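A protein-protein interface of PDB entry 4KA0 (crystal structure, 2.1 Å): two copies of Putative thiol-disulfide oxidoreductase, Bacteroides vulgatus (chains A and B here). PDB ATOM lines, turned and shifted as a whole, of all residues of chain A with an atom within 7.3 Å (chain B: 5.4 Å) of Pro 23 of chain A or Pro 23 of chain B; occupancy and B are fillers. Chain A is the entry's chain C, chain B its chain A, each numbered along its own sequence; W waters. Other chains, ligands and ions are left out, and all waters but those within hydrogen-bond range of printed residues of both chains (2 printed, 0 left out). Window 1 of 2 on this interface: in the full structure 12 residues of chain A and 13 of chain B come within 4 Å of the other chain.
The backbone carbonyl oxygen (O) of Leu 153 of chain A sits close to the side-chain hydroxyl (OG) of Ser 156 of chain A (3.4 Å).
Printed residues of chain B within 4 Å of Asn 139 of chain A: Asn 139. Of the printed residues of chain A, Leu 22 of chain B touches Ser 156. Gly 24 of chain B touches none of the printed residues of chain A. Asn 136 of chain A touches none of the printed residues of chain B. The nearest printed residue of chain B that does not touch Pro 23 of chain A is Gly 24 of chain B (5.8 Å). The nearest printed residue of chain A that does not touch Pro 23 of chain B is Asn 139 of chain A (5.5 Å). The nearest printed residue of chain B that does not touch Asn 139 of chain A is Pro 23 of chain B (5.5 Å).
Water W2 lies within hydrogen-bond range of OD1 of Asn 139 of chain B, OD1 of Asn 139 of chain A and N of Ala 140 of chain A. Water W1 bridges OG of Ser 156 of chain A (2.9 Å) and O of Leu 21 of chain B (3.5 Å).
Pro 23 of chain B touches Pro 23 of chain A. Val 138 of chain B touches Pro 23 of chain A (O to CG, 3.4 Å). CG of Pro 23 of chain A touches ND2 of Asn 139 of chain B, at 3.9 Å. Pro 23 of chain B touches Val 138 of chain A. Asn 139 of chain B touches Val 138 of chain A (ND2 to O, 3.7 Å). Ser 156 of chain A touches Leu 22 of chain B.
ND2 of Asn 139 of chain B lies close to ND2 of Asn 139 of chain A.
Pro 23 of chain A touches its own counterpart, Pro 23 of chain B. Pro 23 of chain A touches Val 138 of chain B, and with the chains exchanged Val 138 of chain A touches Pro 23 of chain B. Pro 23 of chain A touches Asn 139 of chain B, but with the chains exchanged Asn 139 of chain A does not touch Pro 23 of chain B (5.5 Å). Asn 139 of chain B touches its own counterpart, Asn 139 of chain A. Positions printed for both chains: 21, 22, 23, 24, 25, 137, 138 and 139. Of the 7 pairs that touch across the chains among the printed residues, 4 have their exchanged pair printed and touching as well.
Of the 8 printed residues of chain B, 4 touch a printed residue of chain A. Hydrophobic or aromatic side chains of chain B that line the printed part of chain A: Leu 22 and Pro 23. Of the 16 printed residues of chain A, 4 touch a printed residue of chain B. Hydrophobic or aromatic side chains of chain A within 4 Å of the printed part of chain B: Pro 23. Along chain A the printed residues that touch a printed residue of chain B span positions 23 to 156. Among the printed residues, no Asp or Glu carboxylate lies within 4 Å of a Lys or Arg side-chain nitrogen of the other chain.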
ATOM      1  N   SER A  19      18.439 -11.624 -31.541  1.00  0.00           N
ATOM      2  CA  SER A  19      19.102 -11.107 -30.347  1.00  0.00           C
ATOM      3  C   SER A  19      18.216 -11.249 -29.085  1.00  0.00           C
ATOM      4  O   SER A  19      18.644 -10.943 -27.951  1.00  0.00           O
ATOM      5  CB  SER A  19      19.547  -9.662 -30.567  1.00  0.00           C
ATOM      6  OG  SER A  19      20.803  -9.626 -31.266  1.00  0.00           O
ATOM      7  N   LYS A  20      16.997 -11.730 -29.296  1.00  0.00           N
ATOM      8  CA  LYS A  20      16.022 -11.921 -28.242  1.00  0.00           C
ATOM      9  C   LYS A  20      16.337 -13.162 -27.369  1.00  0.00           C
ATOM     10  O   LYS A  20      15.857 -13.276 -26.238  1.00  0.00           O
ATOM     11  CB  LYS A  20      14.647 -12.082 -28.890  1.00  0.00           C
ATOM     12  CG  LYS A  20      13.532 -11.413 -28.128  1.00  0.00           C
ATOM     13  CD  LYS A  20      13.426  -9.927 -28.435  1.00  0.00           C
ATOM     14  CE  LYS A  20      12.034  -9.417 -28.065  1.00  0.00           C
ATOM     15  NZ  LYS A  20      11.826  -7.988 -28.437  1.00  0.00           N
ATOM     16  N   LEU A  21      17.139 -14.073 -27.920  1.00  0.00           N
ATOM     17  CA  LEU A  21      17.503 -15.332 -27.277  1.00  0.00           C
ATOM     18  C   LEU A  21      18.879 -15.354 -26.616  1.00  0.00           C
ATOM     19  O   LEU A  21      19.300 -16.413 -26.130  1.00  0.00           O
ATOM     20  CB  LEU A  21      17.400 -16.495 -28.286  1.00  0.00           C
ATOM     21  CG  LEU A  21      15.981 -16.666 -28.844  1.00  0.00           C
ATOM     22  CD1 LEU A  21      15.839 -17.865 -29.737  1.00  0.00           C
ATOM     23  CD2 LEU A  21      14.944 -16.729 -27.747  1.00  0.00           C
ATOM     24  N   LEU A  22      19.548 -14.202 -26.541  1.00  0.00           N
ATOM     25  CA  LEU A  22      20.877 -14.123 -25.954  1.00  0.00           C
ATOM     26  C   LEU A  22      20.759 -14.230 -24.437  1.00  0.00           C
ATOM     27  O   LEU A  22      19.753 -13.807 -23.870  1.00  0.00           O
ATOM     28  CB  LEU A  22      21.564 -12.802 -26.336  1.00  0.00           C
ATOM     29  CG  LEU A  22      22.211 -12.724 -27.732  1.00  0.00           C
ATOM     30  CD1 LEU A  22      22.724 -11.352 -28.053  1.00  0.00           C
ATOM     31  CD2 LEU A  22      23.369 -13.667 -27.836  1.00  0.00           C
ATOM     32  N   PRO A  23      21.806 -14.748 -23.772  1.00  0.00           N
ATOM     33  CA  PRO A  23      21.836 -14.816 -22.338  1.00  0.00           C
ATOM     34  C   PRO A  23      21.492 -13.479 -21.747  1.00  0.00           C
ATOM     35  O   PRO A  23      21.942 -12.467 -22.247  1.00  0.00           O
ATOM     36  CB  PRO A  23      23.290 -15.214 -22.018  1.00  0.00           C
ATOM     37  CG  PRO A  23      23.708 -15.997 -23.203  1.00  0.00           C
ATOM     38  CD  PRO A  23      23.023 -15.338 -24.365  1.00  0.00           C
ATOM     39  N   GLY A  24      20.668 -13.482 -20.724  1.00  0.00           N
ATOM     40  CA  GLY A  24      20.356 -12.296 -19.991  1.00  0.00           C
ATOM     41  C   GLY A  24      19.086 -11.677 -20.487  1.00  0.00           C
ATOM     42  O   GLY A  24      18.521 -10.846 -19.821  1.00  0.00           O
ATOM     43  N   GLN A  25      18.596 -12.130 -21.626  1.00  0.00           N
ATOM     44  CA  GLN A  25      17.279 -11.706 -22.121  1.00  0.00           C
ATOM     45  C   GLN A  25      16.164 -12.487 -21.518  1.00  0.00           C
ATOM     46  O   GLN A  25      16.338 -13.645 -21.125  1.00  0.00           O
ATOM     47  CB  GLN A  25      17.221 -11.908 -23.623  1.00  0.00           C
ATOM     48  CG  GLN A  25      18.207 -11.019 -24.312  1.00  0.00           C
ATOM     49  CD  GLN A  25      17.832  -9.566 -24.161  1.00  0.00           C
ATOM     50  OE1 GLN A  25      18.587  -8.766 -23.615  1.00  0.00           O
ATOM     51  NE2 GLN A  25      16.643  -9.226 -24.616  1.00  0.00           N
ATOM     52  N   PRO A  26      14.987 -11.867 -21.444  1.00  0.00           N
ATOM     53  CA  PRO A  26      13.894 -12.582 -20.754  1.00  0.00           C
ATOM     54  C   PRO A  26      13.419 -13.844 -21.509  1.00  0.00           C
ATOM     55  O   PRO A  26      13.320 -13.824 -22.697  1.00  0.00           O
ATOM     56  CB  PRO A  26      12.781 -11.522 -20.639  1.00  0.00           C
ATOM     57  CG  PRO A  26      13.122 -10.442 -21.627  1.00  0.00           C
ATOM     58  CD  PRO A  26      14.603 -10.526 -21.936  1.00  0.00           C
ATOM     59  N   ASN A 136      15.347 -15.132 -16.823  1.00  0.00           N
ATOM     60  CA  ASN A 136      16.193 -14.793 -17.931  1.00  0.00           C
ATOM     61  C   ASN A 136      16.951 -16.021 -18.461  1.00  0.00           C
ATOM     62  O   ASN A 136      17.294 -16.955 -17.730  1.00  0.00           O
ATOM     63  CB  ASN A 136      17.155 -13.716 -17.508  1.00  0.00           C
ATOM     64  CG  ASN A 136      16.436 -12.431 -17.124  1.00  0.00           C
ATOM     65  OD1 ASN A 136      15.551 -11.951 -17.841  1.00  0.00           O
ATOM     66  ND2 ASN A 136      16.833 -11.854 -16.008  1.00  0.00           N
ATOM     67  N   ILE A 137      17.231 -15.974 -19.744  1.00  0.00           N
ATOM     68  CA  ILE A 137      17.955 -17.013 -20.410  1.00  0.00           C
ATOM     69  C   ILE A 137      19.376 -17.072 -19.872  1.00  0.00           C
ATOM     70  O   ILE A 137      19.987 -16.022 -19.674  1.00  0.00           O
ATOM     71  CB  ILE A 137      17.914 -16.825 -21.937  1.00  0.00           C
ATOM     72  CG1 ILE A 137      16.458 -16.924 -22.419  1.00  0.00           C
ATOM     73  CG2 ILE A 137      18.781 -17.885 -22.625  1.00  0.00           C
ATOM     74  CD1 ILE A 137      16.226 -16.532 -23.870  1.00  0.00           C
ATOM     75  N   VAL A 138      19.833 -18.298 -19.527  1.00  0.00           N
ATOM     76  CA  VAL A 138      21.235 -18.587 -19.245  1.00  0.00           C
ATOM     77  C   VAL A 138      21.899 -19.037 -20.532  1.00  0.00           C
ATOM     78  O   VAL A 138      22.835 -18.392 -20.984  1.00  0.00           O
ATOM     79  CB  VAL A 138      21.447 -19.636 -18.143  1.00  0.00           C
ATOM     80  CG1 VAL A 138      22.951 -19.808 -17.908  1.00  0.00           C
ATOM     81  CG2 VAL A 138      20.795 -19.164 -16.871  1.00  0.00           C
ATOM     82  N   ASN A 139      21.339 -20.076 -21.148  1.00  0.00           N
ATOM     83  CA  ASN A 139      21.806 -20.604 -22.429  1.00  0.00           C
ATOM     84  C   ASN A 139      20.591 -21.184 -23.160  1.00  0.00           C
ATOM     85  O   ASN A 139      20.073 -22.222 -22.797  1.00  0.00           O
ATOM     86  CB  ASN A 139      22.909 -21.686 -22.200  1.00  0.00           C
ATOM     87  CG  ASN A 139      23.512 -22.289 -23.515  1.00  0.00           C
ATOM     88  OD1 ASN A 139      22.865 -22.366 -24.571  1.00  0.00           O
ATOM     89  ND2 ASN A 139      24.741 -22.805 -23.405  1.00  0.00           N
ATOM     90  N   ALA A 140      20.166 -20.522 -24.216  1.00  0.00           N
ATOM     91  CA  ALA A 140      19.118 -21.021 -25.069  1.00  0.00           C
ATOM     92  C   ALA A 140      19.493 -22.230 -25.893  1.00  0.00           C
ATOM     93  O   ALA A 140      18.615 -22.859 -26.489  1.00  0.00           O
ATOM     94  CB  ALA A 140      18.710 -19.898 -26.007  1.00  0.00           C
ATOM     95  N   LEU A 153      27.266 -26.340 -14.915  1.00  0.00           N
ATOM     96  CA  LEU A 153      26.460 -25.202 -15.361  1.00  0.00           C
ATOM     97  C   LEU A 153      25.350 -24.942 -14.350  1.00  0.00           C
ATOM     98  O   LEU A 153      25.205 -23.827 -13.843  1.00  0.00           O
ATOM     99  CB  LEU A 153      25.890 -25.408 -16.766  1.00  0.00           C
ATOM    100  CG  LEU A 153      25.216 -24.206 -17.432  1.00  0.00           C
ATOM    101  CD1 LEU A 153      26.015 -22.930 -17.268  1.00  0.00           C
ATOM    102  CD2 LEU A 153      24.939 -24.415 -18.913  1.00  0.00           C
ATOM    103  N   SER A 156      26.562 -23.667 -11.084  1.00  0.00           N
ATOM    104  CA  SER A 156      26.829 -22.214 -11.332  1.00  0.00           C
ATOM    105  C   SER A 156      25.624 -21.374 -11.078  1.00  0.00           C
ATOM    106  O   SER A 156      25.721 -20.355 -10.428  1.00  0.00           O
ATOM    107  CB  SER A 156      27.150 -21.914 -12.782  1.00  0.00           C
ATOM    108  OG  SER A 156      28.324 -22.545 -13.155  1.00  0.00           O
ATOM    109  N   VAL A 157      24.486 -21.800 -11.643  1.00  0.00           N
ATOM    110  CA  VAL A 157      23.248 -21.012 -11.648  1.00  0.00           C
ATOM    111  C   VAL A 157      22.513 -21.085 -10.331  1.00  0.00           C
ATOM    112  O   VAL A 157      21.817 -20.145  -9.943  1.00  0.00           O
ATOM    113  CB  VAL A 157      22.282 -21.456 -12.787  1.00  0.00           C
ATOM    114  CG1 VAL A 157      21.083 -20.519 -12.883  1.00  0.00           C
ATOM    115  CG2 VAL A 157      22.993 -21.482 -14.136  1.00  0.00           C
ATOM    116  N   LEU B  21      32.281 -18.425 -14.803  1.00  0.00           N
ATOM    117  CA  LEU B  21      32.030 -18.801 -16.200  1.00  0.00           C
ATOM    118  C   LEU B  21      30.583 -18.551 -16.685  1.00  0.00           C
ATOM    119  O   LEU B  21      30.179 -19.065 -17.704  1.00  0.00           O
ATOM    120  CB  LEU B  21      32.421 -20.272 -16.478  1.00  0.00           C
ATOM    121  CG  LEU B  21      33.832 -20.689 -16.044  1.00  0.00           C
ATOM    122  CD1 LEU B  21      34.055 -22.149 -16.418  1.00  0.00           C
ATOM    123  CD2 LEU B  21      34.902 -19.799 -16.653  1.00  0.00           C
ATOM    124  N   LEU B  22      29.812 -17.755 -15.965  1.00  0.00           N
ATOM    125  CA  LEU B  22      28.460 -17.453 -16.411  1.00  0.00           C
ATOM    126  C   LEU B  22      28.456 -16.427 -17.514  1.00  0.00           C
ATOM    127  O   LEU B  22      29.319 -15.567 -17.584  1.00  0.00           O
ATOM    128  CB  LEU B  22      27.593 -16.973 -15.255  1.00  0.00           C
ATOM    129  CG  LEU B  22      27.094 -18.137 -14.387  1.00  0.00           C
ATOM    130  CD1 LEU B  22      26.620 -17.613 -13.062  1.00  0.00           C
ATOM    131  CD2 LEU B  22      25.993 -18.931 -15.088  1.00  0.00           C
ATOM    132  N   PRO B  23      27.471 -16.505 -18.405  1.00  0.00           N
ATOM    133  CA  PRO B  23      27.378 -15.490 -19.431  1.00  0.00           C
ATOM    134  C   PRO B  23      27.386 -14.096 -18.847  1.00  0.00           C
ATOM    135  O   PRO B  23      26.747 -13.848 -17.843  1.00  0.00           O
ATOM    136  CB  PRO B  23      26.023 -15.770 -20.044  1.00  0.00           C
ATOM    137  CG  PRO B  23      25.884 -17.282 -19.928  1.00  0.00           C
ATOM    138  CD  PRO B  23      26.539 -17.625 -18.617  1.00  0.00           C
ATOM    139  N   GLY B  24      28.093 -13.183 -19.485  1.00  0.00           N
ATOM    140  CA  GLY B  24      28.263 -11.844 -18.946  1.00  0.00           C
ATOM    141  C   GLY B  24      29.530 -11.683 -18.103  1.00  0.00           C
ATOM    142  O   GLY B  24      30.034 -10.597 -17.947  1.00  0.00           O
ATOM    143  N   GLN B  25      30.060 -12.758 -17.574  1.00  0.00           N
ATOM    144  CA  GLN B  25      31.360 -12.687 -16.902  1.00  0.00           C
ATOM    145  C   GLN B  25      32.534 -12.456 -17.877  1.00  0.00           C
ATOM    146  O   GLN B  25      32.487 -12.968 -18.968  1.00  0.00           O
ATOM    147  CB  GLN B  25      31.604 -13.976 -16.131  1.00  0.00           C
ATOM    148  CG  GLN B  25      30.650 -14.153 -14.972  1.00  0.00           C
ATOM    149  CD  GLN B  25      30.696 -12.955 -14.070  1.00  0.00           C
ATOM    150  OE1 GLN B  25      31.724 -12.651 -13.514  1.00  0.00           O
ATOM    151  NE2 GLN B  25      29.590 -12.236 -13.968  1.00  0.00           N
ATOM    152  N   ILE B 137      32.007 -13.387 -21.655  1.00  0.00           N
ATOM    153  CA  ILE B 137      31.497 -14.691 -22.029  1.00  0.00           C
ATOM    154  C   ILE B 137      30.052 -14.545 -22.527  1.00  0.00           C
ATOM    155  O   ILE B 137      29.289 -13.791 -21.950  1.00  0.00           O
ATOM    156  CB  ILE B 137      31.550 -15.667 -20.854  1.00  0.00           C
ATOM    157  CG1 ILE B 137      33.023 -15.858 -20.379  1.00  0.00           C
ATOM    158  CG2 ILE B 137      30.827 -16.966 -21.220  1.00  0.00           C
ATOM    159  CD1 ILE B 137      33.227 -16.873 -19.280  1.00  0.00           C
ATOM    160  N   VAL B 138      29.737 -15.232 -23.633  1.00  0.00           N
ATOM    161  CA  VAL B 138      28.370 -15.357 -24.159  1.00  0.00           C
ATOM    162  C   VAL B 138      27.924 -16.719 -23.741  1.00  0.00           C
ATOM    163  O   VAL B 138      26.981 -16.825 -23.007  1.00  0.00           O
ATOM    164  CB  VAL B 138      28.286 -15.252 -25.698  1.00  0.00           C
ATOM    165  CG1 VAL B 138      26.831 -15.345 -26.154  1.00  0.00           C
ATOM    166  CG2 VAL B 138      28.891 -13.947 -26.176  1.00  0.00           C
ATOM    167  N   ASN B 139      28.610 -17.756 -24.189  1.00  0.00           N
ATOM    168  CA  ASN B 139      28.385 -19.106 -23.696  1.00  0.00           C
ATOM    169  C   ASN B 139      29.690 -19.868 -23.505  1.00  0.00           C
ATOM    170  O   ASN B 139      30.475 -20.064 -24.455  1.00  0.00           O
ATOM    171  CB  ASN B 139      27.493 -19.882 -24.636  1.00  0.00           C
ATOM    172  CG  ASN B 139      26.067 -19.376 -24.573  1.00  0.00           C
ATOM    173  OD1 ASN B 139      25.590 -18.797 -25.535  1.00  0.00           O
ATOM    174  ND2 ASN B 139      25.413 -19.491 -23.373  1.00  0.00           N
HETATM  175  O   HOH W   1      29.465 -21.851 -15.757  1.00  0.00           O
HETATM  176  O   HOH W   2      23.235 -19.564 -25.483  1.00  0.00           O
